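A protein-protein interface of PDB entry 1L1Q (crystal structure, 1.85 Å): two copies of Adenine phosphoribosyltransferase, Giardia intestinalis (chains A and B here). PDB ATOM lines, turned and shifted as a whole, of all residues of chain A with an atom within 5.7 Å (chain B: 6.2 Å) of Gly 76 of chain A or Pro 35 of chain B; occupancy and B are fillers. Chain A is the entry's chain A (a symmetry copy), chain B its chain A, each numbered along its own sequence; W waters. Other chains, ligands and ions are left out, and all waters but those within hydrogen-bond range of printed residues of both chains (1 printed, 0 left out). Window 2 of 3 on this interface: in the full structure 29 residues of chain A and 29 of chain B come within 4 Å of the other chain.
ND2 of Asn 73 of chain A sits at hydrogen-bond distance from OD1 of Asp 39 of chain B (3.1 Å).
Gly 76 of chain A touches just one residue of chain B: Pro 35. Printed residues of chain A within 4 Å of Pro 35 of chain B: Gly 76, Val 77 and Gly 78. Of the printed residues of chain B, Asn 73 of chain A touches Leu 38 (3.8 Å) and Asp 39 (3.1 Å). Printed residues of chain A within 4 Å of Leu 32 of chain B: Gly 78 (3.6 Å). Printed residues of chain B within 4 Å of Val 77 of chain A: Pro 35. Printed residues of chain A within 4 Å of Ser 33 of chain B: Gly 78 (3.4 Å). Of the printed residues of chain B, Gly 78 of chain A touches Leu 32, Ser 33 and Pro 35. Ala 40 of chain B touches none of the printed residues of chain A. The nearest printed residue of chain A that does not touch Leu 38 of chain B is Val 77 of chain A (5.0 Å).
Among the printed residues, pairs that only touch across the chains: Gly 78 of chain A with Ser 33 of chain B, Gly 78 of chain A with Leu 32 of chain B, Gly 76 of chain A with Pro 35 of chain B, Gly 78 of chain A with Pro 35 of chain B, Asn 73 of chain A with Leu 38 of chain B and Val 77 of chain A with Pro 35 of chain B.
No position is printed for both chains.
Water W1 lies within hydrogen-bond range of O of Asn 73 of chain A (2.9 Å) and OD1 of Asp 39 of chain B (2.9 Å).
Along chain B the printed residues that touch a printed residue of chain A span positions 32 to 39. Printed residues of chain A that touch a printed residue of chain B: Asn 73, Gly 76, Val 77 and Gly 78. Among the printed residues, no Asp or Glu carboxylate lies within 4 Å of a Lys or Arg side-chain nitrogen of the other chain.
O of Ile 31 of chain B lies within hydrogen-bond range of N of Leu 38 of chain B (3.4 Å). The backbone NH (N) of Val 77 of chain A is in hydrogen-bond range of the backbone carbonyl oxygen (O) of Ala 72 of chain A (2.9 Å).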
ATOM      1  N   VAL A  71      12.795 -32.392   8.628  1.00  0.00           N
ATOM      2  CA  VAL A  71      11.399 -32.740   8.403  1.00  0.00           C
ATOM      3  C   VAL A  71      10.906 -32.147   7.090  1.00  0.00           C
ATOM      4  O   VAL A  71      10.235 -32.821   6.316  1.00  0.00           O
ATOM      5  CB  VAL A  71      10.519 -32.262   9.580  1.00  0.00           C
ATOM      6  CG1 VAL A  71       9.046 -32.488   9.269  1.00  0.00           C
ATOM      7  CG2 VAL A  71      10.912 -33.016  10.833  1.00  0.00           C
ATOM      8  N   ALA A  72      11.265 -30.896   6.819  1.00  0.00           N
ATOM      9  CA  ALA A  72      10.846 -30.263   5.576  1.00  0.00           C
ATOM     10  C   ALA A  72      11.313 -31.095   4.378  1.00  0.00           C
ATOM     11  O   ALA A  72      10.528 -31.419   3.493  1.00  0.00           O
ATOM     12  CB  ALA A  72      11.437 -28.853   5.480  1.00  0.00           C
ATOM     13  N   ASN A  73      12.595 -31.441   4.354  1.00  0.00           N
ATOM     14  CA  ASN A  73      13.126 -32.196   3.222  1.00  0.00           C
ATOM     15  C   ASN A  73      12.536 -33.599   3.147  1.00  0.00           C
ATOM     16  O   ASN A  73      12.313 -34.117   2.064  1.00  0.00           O
ATOM     17  CB  ASN A  73      14.650 -32.261   3.288  1.00  0.00           C
ATOM     18  CG  ASN A  73      15.279 -32.514   1.921  1.00  0.00           C
ATOM     19  OD1 ASN A  73      15.905 -33.539   1.701  1.00  0.00           O
ATOM     20  ND2 ASN A  73      15.101 -31.573   1.000  1.00  0.00           N
ATOM     21  N   SER A  74      12.270 -34.200   4.300  1.00  0.00           N
ATOM     22  CA  SER A  74      11.692 -35.534   4.339  1.00  0.00           C
ATOM     23  C   SER A  74      10.276 -35.521   3.758  1.00  0.00           C
ATOM     24  O   SER A  74       9.909 -36.405   2.977  1.00  0.00           O
ATOM     25  CB  SER A  74      11.670 -36.041   5.781  1.00  0.00           C
ATOM     26  OG  SER A  74      11.226 -37.384   5.829  1.00  0.00           O
ATOM     27  N   LEU A  75       9.486 -34.516   4.140  1.00  0.00           N
ATOM     28  CA  LEU A  75       8.111 -34.369   3.645  1.00  0.00           C
ATOM     29  C   LEU A  75       8.105 -33.907   2.191  1.00  0.00           C
ATOM     30  O   LEU A  75       7.111 -34.052   1.485  1.00  0.00           O
ATOM     31  CB  LEU A  75       7.346 -33.338   4.484  1.00  0.00           C
ATOM     32  CG  LEU A  75       7.092 -33.690   5.946  1.00  0.00           C
ATOM     33  CD1 LEU A  75       6.454 -32.497   6.632  1.00  0.00           C
ATOM     34  CD2 LEU A  75       6.204 -34.933   6.045  1.00  0.00           C
ATOM     35  N   GLY A  76       9.214 -33.333   1.749  1.00  0.00           N
ATOM     36  CA  GLY A  76       9.292 -32.857   0.384  1.00  0.00           C
ATOM     37  C   GLY A  76       8.680 -31.481   0.220  1.00  0.00           C
ATOM     38  O   GLY A  76       8.114 -31.176  -0.831  1.00  0.00           O
ATOM     39  N   VAL A  77       8.769 -30.649   1.258  1.00  0.00           N
ATOM     40  CA  VAL A  77       8.231 -29.296   1.188  1.00  0.00           C
ATOM     41  C   VAL A  77       9.356 -28.319   1.533  1.00  0.00           C
ATOM     42  O   VAL A  77      10.390 -28.725   2.058  1.00  0.00           O
ATOM     43  CB  VAL A  77       7.046 -29.076   2.192  1.00  0.00           C
ATOM     44  CG1 VAL A  77       5.913 -30.066   1.901  1.00  0.00           C
ATOM     45  CG2 VAL A  77       7.529 -29.233   3.628  1.00  0.00           C
ATOM     46  N   GLY A  78       9.147 -27.041   1.248  1.00  0.00           N
ATOM     47  CA  GLY A  78      10.166 -26.050   1.552  1.00  0.00           C
ATOM     48  C   GLY A  78      10.223 -25.691   3.023  1.00  0.00           C
ATOM     49  O   GLY A  78       9.255 -25.890   3.758  1.00  0.00           O
ATOM     50  N   ASP B  30      15.298 -18.433  -0.650  1.00  0.00           N
ATOM     51  CA  ASP B  30      14.425 -19.042  -1.641  1.00  0.00           C
ATOM     52  C   ASP B  30      14.865 -20.444  -2.093  1.00  0.00           C
ATOM     53  O   ASP B  30      14.064 -21.202  -2.622  1.00  0.00           O
ATOM     54  CB  ASP B  30      14.233 -18.079  -2.810  1.00  0.00           C
ATOM     55  CG  ASP B  30      13.653 -16.728  -2.362  1.00  0.00           C
ATOM     56  OD1 ASP B  30      12.617 -16.711  -1.672  1.00  0.00           O
ATOM     57  OD2 ASP B  30      14.233 -15.669  -2.691  1.00  0.00           O
ATOM     58  N   ILE B  31      16.122 -20.807  -1.865  1.00  0.00           N
ATOM     59  CA  ILE B  31      16.571 -22.161  -2.210  1.00  0.00           C
ATOM     60  C   ILE B  31      15.967 -23.088  -1.148  1.00  0.00           C
ATOM     61  O   ILE B  31      15.458 -24.169  -1.447  1.00  0.00           O
ATOM     62  CB  ILE B  31      18.109 -22.288  -2.141  1.00  0.00           C
ATOM     63  CG1 ILE B  31      18.747 -21.512  -3.291  1.00  0.00           C
ATOM     64  CG2 ILE B  31      18.531 -23.758  -2.207  1.00  0.00           C
ATOM     65  CD1 ILE B  31      20.266 -21.460  -3.223  1.00  0.00           C
ATOM     66  N   LEU B  32      16.011 -22.637   0.100  1.00  0.00           N
ATOM     67  CA  LEU B  32      15.492 -23.431   1.208  1.00  0.00           C
ATOM     68  C   LEU B  32      13.972 -23.608   1.203  1.00  0.00           C
ATOM     69  O   LEU B  32      13.476 -24.644   1.655  1.00  0.00           O
ATOM     70  CB  LEU B  32      15.926 -22.817   2.545  1.00  0.00           C
ATOM     71  CG  LEU B  32      17.426 -22.519   2.720  1.00  0.00           C
ATOM     72  CD1 LEU B  32      17.650 -21.860   4.078  1.00  0.00           C
ATOM     73  CD2 LEU B  32      18.233 -23.797   2.611  1.00  0.00           C
ATOM     74  N   SER B  33      13.235 -22.616   0.702  1.00  0.00           N
ATOM     75  CA  SER B  33      11.773 -22.687   0.690  1.00  0.00           C
ATOM     76  C   SER B  33      11.222 -23.311  -0.579  1.00  0.00           C
ATOM     77  O   SER B  33      10.014 -23.465  -0.720  1.00  0.00           O
ATOM     78  CB  SER B  33      11.159 -21.294   0.858  1.00  0.00           C
ATOM     79  OG  SER B  33      11.468 -20.438  -0.233  1.00  0.00           O
ATOM     80  N   THR B  34      12.110 -23.661  -1.504  1.00  0.00           N
ATOM     81  CA  THR B  34      11.699 -24.271  -2.768  1.00  0.00           C
ATOM     82  C   THR B  34      12.239 -25.698  -2.774  1.00  0.00           C
ATOM     83  O   THR B  34      13.404 -25.915  -3.077  1.00  0.00           O
ATOM     84  CB  THR B  34      12.283 -23.478  -3.965  1.00  0.00           C
ATOM     85  OG1 THR B  34      11.903 -22.101  -3.846  1.00  0.00           O
ATOM     86  CG2 THR B  34      11.736 -24.018  -5.298  1.00  0.00           C
ATOM     87  N   PRO B  35      11.387 -26.694  -2.462  1.00  0.00           N
ATOM     88  CA  PRO B  35      11.836 -28.091  -2.430  1.00  0.00           C
ATOM     89  C   PRO B  35      12.698 -28.624  -3.573  1.00  0.00           C
ATOM     90  O   PRO B  35      13.686 -29.332  -3.316  1.00  0.00           O
ATOM     91  CB  PRO B  35      10.534 -28.888  -2.244  1.00  0.00           C
ATOM     92  CG  PRO B  35       9.460 -27.968  -2.736  1.00  0.00           C
ATOM     93  CD  PRO B  35       9.929 -26.603  -2.275  1.00  0.00           C
ATOM     94  N   ALA B  36      12.355 -28.304  -4.819  1.00  0.00           N
ATOM     95  CA  ALA B  36      13.157 -28.810  -5.938  1.00  0.00           C
ATOM     96  C   ALA B  36      14.570 -28.219  -5.909  1.00  0.00           C
ATOM     97  O   ALA B  36      15.530 -28.899  -6.238  1.00  0.00           O
ATOM     98  CB  ALA B  36      12.471 -28.510  -7.270  1.00  0.00           C
ATOM     99  N   ALA B  37      14.701 -26.964  -5.491  1.00  0.00           N
ATOM    100  CA  ALA B  37      16.021 -26.329  -5.412  1.00  0.00           C
ATOM    101  C   ALA B  37      16.815 -26.903  -4.232  1.00  0.00           C
ATOM    102  O   ALA B  37      18.018 -27.142  -4.329  1.00  0.00           O
ATOM    103  CB  ALA B  37      15.868 -24.814  -5.260  1.00  0.00           C
ATOM    104  N   LEU B  38      16.138 -27.111  -3.106  1.00  0.00           N
ATOM    105  CA  LEU B  38      16.798 -27.682  -1.940  1.00  0.00           C
ATOM    106  C   LEU B  38      17.243 -29.123  -2.252  1.00  0.00           C
ATOM    107  O   LEU B  38      18.327 -29.543  -1.844  1.00  0.00           O
ATOM    108  CB  LEU B  38      15.849 -27.645  -0.739  1.00  0.00           C
ATOM    109  CG  LEU B  38      16.400 -28.073   0.630  1.00  0.00           C
ATOM    110  CD1 LEU B  38      17.675 -27.323   0.949  1.00  0.00           C
ATOM    111  CD2 LEU B  38      15.342 -27.806   1.706  1.00  0.00           C
ATOM    112  N   ASP B  39      16.416 -29.886  -2.970  1.00  0.00           N
ATOM    113  CA  ASP B  39      16.798 -31.259  -3.325  1.00  0.00           C
ATOM    114  C   ASP B  39      18.038 -31.238  -4.228  1.00  0.00           C
ATOM    115  O   ASP B  39      18.965 -32.015  -4.034  1.00  0.00           O
ATOM    116  CB  ASP B  39      15.676 -31.988  -4.079  1.00  0.00           C
ATOM    117  CG  ASP B  39      14.517 -32.397  -3.179  1.00  0.00           C
ATOM    118  OD1 ASP B  39      14.668 -32.400  -1.946  1.00  0.00           O
ATOM    119  OD2 ASP B  39      13.443 -32.726  -3.722  1.00  0.00           O
ATOM    120  N   ALA B  40      18.041 -30.352  -5.221  1.00  0.00           N
ATOM    121  CA  ALA B  40      19.166 -30.251  -6.144  1.00  0.00           C
ATOM    122  C   ALA B  40      20.488 -30.023  -5.407  1.00  0.00           C
ATOM    123  O   ALA B  40      21.492 -30.680  -5.686  1.00  0.00           O
ATOM    124  CB  ALA B  40      18.925 -29.121  -7.137  1.00  0.00           C
HETATM  125  O   HOH W   1      12.229 -32.619  -0.363  1.00  0.00           O
